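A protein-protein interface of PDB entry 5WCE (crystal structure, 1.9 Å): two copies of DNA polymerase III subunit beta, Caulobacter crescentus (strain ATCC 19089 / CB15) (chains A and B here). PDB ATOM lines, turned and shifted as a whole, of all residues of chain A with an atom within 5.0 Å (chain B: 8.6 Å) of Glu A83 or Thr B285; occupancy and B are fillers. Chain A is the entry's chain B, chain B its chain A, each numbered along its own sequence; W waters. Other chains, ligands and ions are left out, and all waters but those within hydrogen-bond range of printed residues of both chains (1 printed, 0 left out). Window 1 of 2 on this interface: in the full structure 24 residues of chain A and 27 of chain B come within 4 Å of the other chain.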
ATOM      1  N   HIS A  79     -24.675   6.287  -6.067  1.00  0.00           N
ATOM      2  CA  HIS A  79     -25.441   7.533  -5.877  1.00  0.00           C
ATOM      3  C   HIS A  79     -25.283   8.032  -4.429  1.00  0.00           C
ATOM      4  O   HIS A  79     -25.101   9.215  -4.196  1.00  0.00           O
ATOM      5  CB  HIS A  79     -26.938   7.352  -6.203  1.00  0.00           C
ATOM      6  CG  HIS A  79     -27.230   7.029  -7.641  1.00  0.00           C
ATOM      7  ND1 HIS A  79     -26.707   7.752  -8.689  1.00  0.00           N
ATOM      8  CD2 HIS A  79     -28.039   6.096  -8.196  1.00  0.00           C
ATOM      9  CE1 HIS A  79     -27.128   7.236  -9.829  1.00  0.00           C
ATOM     10  NE2 HIS A  79     -27.947   6.240  -9.551  1.00  0.00           N
ATOM     11  N   THR A  80     -25.311   7.110  -3.485  1.00  0.00           N
ATOM     12  CA  THR A  80     -25.108   7.460  -2.081  1.00  0.00           C
ATOM     13  C   THR A  80     -23.755   8.099  -1.812  1.00  0.00           C
ATOM     14  O   THR A  80     -23.653   9.167  -1.154  1.00  0.00           O
ATOM     15  CB  THR A  80     -25.342   6.269  -1.169  1.00  0.00           C
ATOM     16  OG1 THR A  80     -26.696   5.857  -1.337  1.00  0.00           O
ATOM     17  CG2 THR A  80     -25.085   6.614   0.295  1.00  0.00           C
ATOM     18  N   LEU A  81     -22.710   7.460  -2.326  1.00  0.00           N
ATOM     19  CA  LEU A  81     -21.408   8.054  -2.237  1.00  0.00           C
ATOM     20  C   LEU A  81     -21.332   9.434  -2.866  1.00  0.00           C
ATOM     21  O   LEU A  81     -20.838  10.367  -2.228  1.00  0.00           O
ATOM     22  CB  LEU A  81     -20.347   7.134  -2.811  1.00  0.00           C
ATOM     23  CG  LEU A  81     -18.900   7.504  -2.607  1.00  0.00           C
ATOM     24  CD1 LEU A  81     -18.532   7.760  -1.176  1.00  0.00           C
ATOM     25  CD2 LEU A  81     -18.035   6.360  -3.174  1.00  0.00           C
ATOM     26  N   TYR A  82     -21.885   9.570  -4.067  1.00  0.00           N
ATOM     27  CA  TYR A  82     -21.918  10.861  -4.775  1.00  0.00           C
ATOM     28  C   TYR A  82     -22.656  11.945  -3.926  1.00  0.00           C
ATOM     29  O   TYR A  82     -22.144  13.040  -3.710  1.00  0.00           O
ATOM     30  CB  TYR A  82     -22.582  10.715  -6.156  1.00  0.00           C
ATOM     31  CG  TYR A  82     -22.802  12.035  -6.856  1.00  0.00           C
ATOM     32  CD1 TYR A  82     -21.750  12.756  -7.423  1.00  0.00           C
ATOM     33  CD2 TYR A  82     -24.077  12.595  -6.901  1.00  0.00           C
ATOM     34  CE1 TYR A  82     -21.970  13.982  -8.027  1.00  0.00           C
ATOM     35  CE2 TYR A  82     -24.322  13.812  -7.536  1.00  0.00           C
ATOM     36  CZ  TYR A  82     -23.271  14.488  -8.099  1.00  0.00           C
ATOM     37  OH  TYR A  82     -23.512  15.694  -8.723  1.00  0.00           O
ATOM     38  N   GLU A  83     -23.804  11.605  -3.395  1.00  0.00           N
ATOM     39  CA  GLU A  83     -24.599  12.556  -2.617  1.00  0.00           C
ATOM     40  C   GLU A  83     -23.922  12.974  -1.323  1.00  0.00           C
ATOM     41  O   GLU A  83     -23.943  14.150  -0.957  1.00  0.00           O
ATOM     42  CB  GLU A  83     -25.999  12.005  -2.377  1.00  0.00           C
ATOM     43  CG  GLU A  83     -26.831  11.996  -3.637  1.00  0.00           C
ATOM     44  CD  GLU A  83     -27.121  13.384  -4.168  1.00  0.00           C
ATOM     45  OE1 GLU A  83     -27.481  14.265  -3.391  1.00  0.00           O
ATOM     46  OE2 GLU A  83     -27.047  13.515  -5.378  1.00  0.00           O
ATOM     47  N   ILE A  84     -23.297  12.027  -0.638  1.00  0.00           N
ATOM     48  CA  ILE A  84     -22.527  12.341   0.556  1.00  0.00           C
ATOM     49  C   ILE A  84     -21.449  13.375   0.215  1.00  0.00           C
ATOM     50  O   ILE A  84     -21.295  14.407   0.888  1.00  0.00           O
ATOM     51  CB  ILE A  84     -21.872  11.074   1.181  1.00  0.00           C
ATOM     52  CG1 ILE A  84     -22.914  10.138   1.827  1.00  0.00           C
ATOM     53  CG2 ILE A  84     -20.795  11.451   2.216  1.00  0.00           C
ATOM     54  CD1 ILE A  84     -22.303   8.759   2.120  1.00  0.00           C
ATOM     55  N   VAL A  85     -20.677  13.084  -0.814  1.00  0.00           N
ATOM     56  CA  VAL A  85     -19.551  13.944  -1.116  1.00  0.00           C
ATOM     57  C   VAL A  85     -19.996  15.351  -1.535  1.00  0.00           C
ATOM     58  O   VAL A  85     -19.398  16.344  -1.096  1.00  0.00           O
ATOM     59  CB  VAL A  85     -18.566  13.313  -2.138  1.00  0.00           C
ATOM     60  CG1 VAL A  85     -17.437  14.285  -2.438  1.00  0.00           C
ATOM     61  CG2 VAL A  85     -17.992  12.036  -1.563  1.00  0.00           C
ATOM     62  N   ARG A  86     -21.041  15.400  -2.334  1.00  0.00           N
ATOM     63  CA  ARG A  86     -21.638  16.660  -2.719  1.00  0.00           C
ATOM     64  C   ARG A  86     -21.995  17.554  -1.502  1.00  0.00           C
ATOM     65  O   ARG A  86     -21.824  18.755  -1.540  1.00  0.00           O
ATOM     66  CB  ARG A  86     -22.880  16.393  -3.548  1.00  0.00           C
ATOM     67  CG  ARG A  86     -23.297  17.540  -4.436  1.00  0.00           C
ATOM     68  CD  ARG A  86     -24.542  17.169  -5.273  1.00  0.00           C
ATOM     69  NE  ARG A  86     -25.663  16.796  -4.404  1.00  0.00           N
ATOM     70  CZ  ARG A  86     -26.337  17.640  -3.595  1.00  0.00           C
ATOM     71  NH1 ARG A  86     -26.037  18.941  -3.481  1.00  0.00           N
ATOM     72  NH2 ARG A  86     -27.318  17.149  -2.838  1.00  0.00           N
ATOM     73  N   LYS A  87     -22.452  16.950  -0.422  1.00  0.00           N
ATOM     74  CA  LYS A  87     -22.875  17.700   0.741  1.00  0.00           C
ATOM     75  C   LYS A  87     -21.769  17.978   1.709  1.00  0.00           C
ATOM     76  O   LYS A  87     -21.989  18.722   2.670  1.00  0.00           O
ATOM     77  CB  LYS A  87     -24.022  16.963   1.436  1.00  0.00           C
ATOM     78  CG  LYS A  87     -25.255  16.888   0.520  1.00  0.00           C
ATOM     79  CD  LYS A  87     -26.299  16.037   1.189  1.00  0.00           C
ATOM     80  CE  LYS A  87     -27.629  15.890   0.448  1.00  0.00           C
ATOM     81  NZ  LYS A  87     -28.438  14.925   1.298  1.00  0.00           N
ATOM     82  N   LYS B 278     -27.118  22.010   7.561  1.00  0.00           N
ATOM     83  CA  LYS B 278     -26.176  21.340   6.659  1.00  0.00           C
ATOM     84  C   LYS B 278     -25.766  20.001   7.183  1.00  0.00           C
ATOM     85  O   LYS B 278     -25.663  19.046   6.404  1.00  0.00           O
ATOM     86  CB  LYS B 278     -24.954  22.215   6.344  1.00  0.00           C
ATOM     87  CG  LYS B 278     -25.316  23.261   5.312  1.00  0.00           C
ATOM     88  CD  LYS B 278     -24.212  24.282   5.175  1.00  0.00           C
ATOM     89  CE  LYS B 278     -24.601  25.312   4.133  1.00  0.00           C
ATOM     90  NZ  LYS B 278     -23.622  26.412   4.302  1.00  0.00           N
ATOM     91  N   ALA B 279     -25.584  19.916   8.501  1.00  0.00           N
ATOM     92  CA  ALA B 279     -25.230  18.659   9.144  1.00  0.00           C
ATOM     93  C   ALA B 279     -26.366  17.669   9.076  1.00  0.00           C
ATOM     94  O   ALA B 279     -26.126  16.531   8.725  1.00  0.00           O
ATOM     95  CB  ALA B 279     -24.775  18.864  10.574  1.00  0.00           C
ATOM     96  N   VAL B 280     -27.588  18.076   9.421  1.00  0.00           N
ATOM     97  CA  VAL B 280     -28.749  17.210   9.272  1.00  0.00           C
ATOM     98  C   VAL B 280     -28.875  16.689   7.835  1.00  0.00           C
ATOM     99  O   VAL B 280     -29.093  15.521   7.624  1.00  0.00           O
ATOM    100  CB  VAL B 280     -30.069  17.907   9.656  1.00  0.00           C
ATOM    101  CG1 VAL B 280     -31.269  16.999   9.382  1.00  0.00           C
ATOM    102  CG2 VAL B 280     -30.046  18.284  11.146  1.00  0.00           C
ATOM    103  N   ASP B 281     -28.798  17.593   6.872  1.00  0.00           N
ATOM    104  CA  ASP B 281     -28.866  17.240   5.469  1.00  0.00           C
ATOM    105  C   ASP B 281     -27.763  16.246   5.072  1.00  0.00           C
ATOM    106  O   ASP B 281     -28.046  15.240   4.397  1.00  0.00           O
ATOM    107  CB  ASP B 281     -28.797  18.531   4.652  1.00  0.00           C
ATOM    108  CG  ASP B 281     -29.064  18.317   3.178  1.00  0.00           C
ATOM    109  OD1 ASP B 281     -29.802  17.397   2.826  1.00  0.00           O
ATOM    110  OD2 ASP B 281     -28.484  19.071   2.384  1.00  0.00           O
ATOM    111  N   ARG B 282     -26.531  16.469   5.531  1.00  0.00           N
ATOM    112  CA  ARG B 282     -25.462  15.510   5.302  1.00  0.00           C
ATOM    113  C   ARG B 282     -25.757  14.106   5.803  1.00  0.00           C
ATOM    114  O   ARG B 282     -25.678  13.129   5.034  1.00  0.00           O
ATOM    115  CB  ARG B 282     -24.142  15.952   5.941  1.00  0.00           C
ATOM    116  CG  ARG B 282     -23.254  16.720   5.041  1.00  0.00           C
ATOM    117  CD  ARG B 282     -21.889  16.883   5.641  1.00  0.00           C
ATOM    118  NE  ARG B 282     -21.944  17.815   6.767  1.00  0.00           N
ATOM    119  CZ  ARG B 282     -21.981  19.142   6.679  1.00  0.00           C
ATOM    120  NH1 ARG B 282     -21.978  19.758   5.501  1.00  0.00           N
ATOM    121  NH2 ARG B 282     -22.022  19.858   7.804  1.00  0.00           N
ATOM    122  N   VAL B 283     -26.070  13.987   7.106  1.00  0.00           N
ATOM    123  CA  VAL B 283     -26.246  12.657   7.696  1.00  0.00           C
ATOM    124  C   VAL B 283     -27.468  11.953   7.116  1.00  0.00           C
ATOM    125  O   VAL B 283     -27.453  10.728   7.009  1.00  0.00           O
ATOM    126  CB  VAL B 283     -26.278  12.680   9.225  1.00  0.00           C
ATOM    127  CG1 VAL B 283     -24.930  13.120   9.767  1.00  0.00           C
ATOM    128  CG2 VAL B 283     -27.383  13.541   9.771  1.00  0.00           C
ATOM    129  N   ALA B 284     -28.482  12.709   6.702  1.00  0.00           N
ATOM    130  CA  ALA B 284     -29.681  12.124   6.087  1.00  0.00           C
ATOM    131  C   ALA B 284     -29.457  11.542   4.666  1.00  0.00           C
ATOM    132  O   ALA B 284     -30.229  10.711   4.208  1.00  0.00           O
ATOM    133  CB  ALA B 284     -30.804  13.145   6.039  1.00  0.00           C
ATOM    134  N   THR B 285     -28.407  12.011   4.015  1.00  0.00           N
ATOM    135  CA  THR B 285     -27.958  11.471   2.761  1.00  0.00           C
ATOM    136  C   THR B 285     -27.686  10.013   2.705  1.00  0.00           C
ATOM    137  O   THR B 285     -27.669   9.489   1.579  1.00  0.00           O
ATOM    138  CB  THR B 285     -26.632  12.090   2.309  1.00  0.00           C
ATOM    139  OG1 THR B 285     -26.767  13.504   2.376  1.00  0.00           O
ATOM    140  CG2 THR B 285     -26.326  11.770   0.857  1.00  0.00           C
ATOM    141  N   ILE B 286     -27.379   9.343   3.806  1.00  0.00           N
ATOM    142  CA  ILE B 286     -27.139   7.874   3.658  1.00  0.00           C
ATOM    143  C   ILE B 286     -28.441   7.133   3.324  1.00  0.00           C
ATOM    144  O   ILE B 286     -28.342   5.958   2.990  1.00  0.00           O
ATOM    145  CB  ILE B 286     -26.418   7.064   4.801  1.00  0.00           C
ATOM    146  CG1 ILE B 286     -26.933   7.415   6.135  1.00  0.00           C
ATOM    147  CG2 ILE B 286     -24.878   7.059   4.709  1.00  0.00           C
ATOM    148  CD1 ILE B 286     -28.400   7.331   6.287  1.00  0.00           C
ATOM    149  N   SER B 287     -29.625   7.761   3.425  1.00  0.00           N
ATOM    150  CA  SER B 287     -30.874   7.074   3.136  1.00  0.00           C
ATOM    151  C   SER B 287     -31.464   7.677   1.843  1.00  0.00           C
ATOM    152  O   SER B 287     -31.584   8.903   1.698  1.00  0.00           O
ATOM    153  CB  SER B 287     -31.847   7.170   4.350  1.00  0.00           C
ATOM    154  OG  SER B 287     -33.134   6.784   3.978  1.00  0.00           O
ATOM    155  N   ALA B 288     -31.805   6.805   0.903  1.00  0.00           N
ATOM    156  CA  ALA B 288     -32.593   7.179  -0.270  1.00  0.00           C
ATOM    157  C   ALA B 288     -34.090   6.998   0.031  1.00  0.00           C
ATOM    158  O   ALA B 288     -34.912   7.283  -0.832  1.00  0.00           O
ATOM    159  CB  ALA B 288     -32.165   6.357  -1.490  1.00  0.00           C
ATOM    160  N   GLU B 289     -34.435   6.557   1.252  1.00  0.00           N
ATOM    161  CA  GLU B 289     -35.822   6.271   1.650  1.00  0.00           C
ATOM    162  C   GLU B 289     -36.615   7.579   1.741  1.00  0.00           C
ATOM    163  O   GLU B 289     -36.052   8.599   2.131  1.00  0.00           O
ATOM    164  CB  GLU B 289     -35.866   5.537   3.011  1.00  0.00           C
ATOM    165  CG  GLU B 289     -34.951   4.318   3.134  1.00  0.00           C
ATOM    166  N   ARG B 292     -37.041   9.474   6.445  1.00  0.00           N
ATOM    167  CA  ARG B 292     -35.698   9.355   6.999  1.00  0.00           C
ATOM    168  C   ARG B 292     -35.783   9.947   8.401  1.00  0.00           C
ATOM    169  O   ARG B 292     -36.100  11.083   8.521  1.00  0.00           O
ATOM    170  CB  ARG B 292     -34.651  10.210   6.208  1.00  0.00           C
ATOM    171  CG  ARG B 292     -34.484   9.953   4.713  1.00  0.00           C
ATOM    172  CD  ARG B 292     -35.178  10.999   3.846  1.00  0.00           C
ATOM    173  NE  ARG B 292     -34.407  12.222   3.594  1.00  0.00           N
ATOM    174  CZ  ARG B 292     -34.718  13.392   4.134  1.00  0.00           C
ATOM    175  NH1 ARG B 292     -35.731  13.454   4.944  1.00  0.00           N
ATOM    176  NH2 ARG B 292     -34.032  14.489   3.874  1.00  0.00           N
ATOM    177  N   VAL B 307     -27.990   9.063  11.580  1.00  0.00           N
ATOM    178  CA  VAL B 307     -28.982   8.502  10.651  1.00  0.00           C
ATOM    179  C   VAL B 307     -28.488   7.120  10.239  1.00  0.00           C
ATOM    180  O   VAL B 307     -27.268   6.889  10.145  1.00  0.00           O
ATOM    181  CB  VAL B 307     -29.196   9.377   9.398  1.00  0.00           C
ATOM    182  CG1 VAL B 307     -30.180   8.771   8.352  1.00  0.00           C
ATOM    183  CG2 VAL B 307     -29.750  10.717   9.767  1.00  0.00           C
ATOM    184  N   ARG B 308     -29.424   6.177  10.106  1.00  0.00           N
ATOM    185  CA  ARG B 308     -29.186   4.841   9.599  1.00  0.00           C
ATOM    186  C   ARG B 308     -30.205   4.574   8.492  1.00  0.00           C
ATOM    187  O   ARG B 308     -31.314   5.086   8.527  1.00  0.00           O
ATOM    188  CB  ARG B 308     -29.300   3.779  10.679  1.00  0.00           C
ATOM    189  CG  ARG B 308     -28.285   3.981  11.813  1.00  0.00           C
ATOM    190  CD  ARG B 308     -28.165   2.790  12.760  1.00  0.00           C
ATOM    191  NE  ARG B 308     -26.910   2.029  12.624  1.00  0.00           N
ATOM    192  CZ  ARG B 308     -26.627   1.141  11.659  1.00  0.00           C
ATOM    193  NH1 ARG B 308     -27.469   0.858  10.669  1.00  0.00           N
ATOM    194  NH2 ARG B 308     -25.462   0.527  11.680  1.00  0.00           N
ATOM    195  N   ASN B 309     -29.799   3.828   7.473  1.00  0.00           N
ATOM    196  CA  ASN B 309     -30.738   3.404   6.456  1.00  0.00           C
ATOM    197  C   ASN B 309     -31.094   1.938   6.710  1.00  0.00           C
ATOM    198  O   ASN B 309     -30.563   1.297   7.645  1.00  0.00           O
ATOM    199  CB  ASN B 309     -30.182   3.661   5.034  1.00  0.00           C
ATOM    200  CG  ASN B 309     -28.941   2.831   4.699  1.00  0.00           C
ATOM    201  OD1 ASN B 309     -28.651   1.798   5.330  1.00  0.00           O
ATOM    202  ND2 ASN B 309     -28.214   3.267   3.699  1.00  0.00           N
ATOM    203  N   GLY B 313     -26.223   1.077   6.328  1.00  0.00           N
ATOM    204  CA  GLY B 313     -25.432   2.296   6.291  1.00  0.00           C
ATOM    205  C   GLY B 313     -25.673   3.187   7.487  1.00  0.00           C
ATOM    206  O   GLY B 313     -26.806   3.337   7.902  1.00  0.00           O
ATOM    207  N   GLN B 314     -24.616   3.805   7.999  1.00  0.00           N
ATOM    208  CA  GLN B 314     -24.681   4.760   9.120  1.00  0.00           C
ATOM    209  C   GLN B 314     -24.016   6.112   8.764  1.00  0.00           C
ATOM    210  O   GLN B 314     -23.022   6.136   8.028  1.00  0.00           O
ATOM    211  CB  GLN B 314     -23.910   4.177  10.292  1.00  0.00           C
ATOM    212  CG  GLN B 314     -23.992   4.999  11.546  1.00  0.00           C
ATOM    213  CD  GLN B 314     -23.065   4.468  12.646  1.00  0.00           C
ATOM    214  OE1 GLN B 314     -23.104   3.287  12.958  1.00  0.00           O
ATOM    215  NE2 GLN B 314     -22.245   5.349  13.255  1.00  0.00           N
ATOM    216  N   ALA B 315     -24.552   7.209   9.318  1.00  0.00           N
ATOM    217  CA  ALA B 315     -23.925   8.537   9.243  1.00  0.00           C
ATOM    218  C   ALA B 315     -24.018   9.257  10.553  1.00  0.00           C
ATOM    219  O   ALA B 315     -25.136   9.376  11.118  1.00  0.00           O
ATOM    220  CB  ALA B 315     -24.597   9.363   8.180  1.00  0.00           C
ATOM    221  N   ALA B 334     -36.233  13.704   9.480  1.00  0.00           N
ATOM    222  CA  ALA B 334     -35.226  14.657   8.981  1.00  0.00           C
ATOM    223  C   ALA B 334     -35.813  15.747   8.099  1.00  0.00           C
ATOM    224  O   ALA B 334     -35.425  16.914   8.229  1.00  0.00           O
ATOM    225  CB  ALA B 334     -34.070  13.950   8.267  1.00  0.00           C
ATOM    226  N   ARG B 335     -36.750  15.388   7.226  1.00  0.00           N
ATOM    227  CA  ARG B 335     -37.374  16.364   6.347  1.00  0.00           C
ATOM    228  C   ARG B 335     -38.142  17.428   7.158  1.00  0.00           C
ATOM    229  O   ARG B 335     -38.039  18.636   6.902  1.00  0.00           O
ATOM    230  CB  ARG B 335     -38.314  15.681   5.296  1.00  0.00           C
ATOM    231  CG  ARG B 335     -39.025  16.654   4.341  1.00  0.00           C
ATOM    232  CD  ARG B 335     -38.108  17.705   3.728  1.00  0.00           C
ATOM    233  NE  ARG B 335     -36.915  17.110   3.114  1.00  0.00           N
ATOM    234  CZ  ARG B 335     -35.763  17.744   2.806  1.00  0.00           C
ATOM    235  NH1 ARG B 335     -35.599  19.045   3.050  1.00  0.00           N
ATOM    236  NH2 ARG B 335     -34.755  17.050   2.240  1.00  0.00           N
ATOM    237  N   LEU B 338     -35.577  19.741   8.744  1.00  0.00           N
ATOM    238  CA  LEU B 338     -35.042  20.632   7.690  1.00  0.00           C
ATOM    239  C   LEU B 338     -36.063  21.645   7.256  1.00  0.00           C
ATOM    240  O   LEU B 338     -35.706  22.785   6.991  1.00  0.00           O
ATOM    241  CB  LEU B 338     -34.509  19.817   6.521  1.00  0.00           C
ATOM    242  CG  LEU B 338     -33.235  19.068   6.858  1.00  0.00           C
ATOM    243  CD1 LEU B 338     -32.955  18.099   5.739  1.00  0.00           C
ATOM    244  CD2 LEU B 338     -32.075  20.030   7.105  1.00  0.00           C
HETATM  245  O   HOH W   1     -23.447  20.834   2.525  1.00  0.00           O
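The side-chain carboxylate of Asp B281 is in salt-bridge range of the side-chain amino group of Lys A87, 3.2 Å away. The guanidinium group (NH1) of Arg B282 is in hydrogen-bond range of the backbone carbonyl oxygen (O) of Lys A87 (3.0 Å). OG1 of Thr B285 lies within hydrogen-bond range of NZ of Lys A87, at 2.4 Å.
O of Asp B281 sits at hydrogen-bond distance from OG1 of Thr B285 (3.0 Å). The backbone carbonyl oxygen of Arg B282 is in hydrogen-bond range of the side-chain hydroxyl of Thr B285 (2.9 Å). OE1 of Glu A83 lies within salt-bridge range of NH2 of Arg A86 (2.9 Å).
Among the printed residues, merely in contact across the chains: Glu A83 with Thr B285 (3.3 Å) and Ile A84 with Thr B285 (3.4 Å).
Glu A83 touches just one residue of chain B: Thr B285 (3.3 Å). Thr B285 touches just these residues of chain A: Glu A83 (3.3 Å), Ile A84 (3.4 Å) and Lys A87 (2.4 Å). Of the printed residues of chain B, Lys A87 touches Asp B281 (3.1 Å), Arg B282 (3.0 Å) and Thr B285 (2.4 Å). Of the printed residues of chain A, Asp B281 touches Lys A87 (3.1 Å). Val B280 touches none of the printed residues of chain A. Val B283 touches none of the printed residues of chain A. The nearest residue of chain B that does not touch Glu A83 is Arg B282 (6.3 Å). The nearest residue of chain A that does not touch Thr B285 is Thr A80 (4.1 Å). The nearest printed residue of chain B that does not touch Ile A84 is Ile B286 (4.03 Å).
Printed residues of chain A that touch a printed residue of chain B: Glu A83, Ile A84 and Lys A87. Hydrophobic or aromatic side chains of chain A within 4 Å of the printed part of chain B: Ile A84. Of the 22 printed residues of chain B, 3 touch a printed residue of chain A. Among the printed residues, 5 pairs touch across the chains. Among the printed residues, Asp or Glu carboxylates within 4 Å of a Lys or Arg side-chain nitrogen of the other chain: Lys A87 with Asp B281 (3.2 Å).
No position is printed for both chains.
Water W1 lies within hydrogen-bond range of O of Lys A87 (2.6 Å) and NH1 of Arg B282 (3.5 Å).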
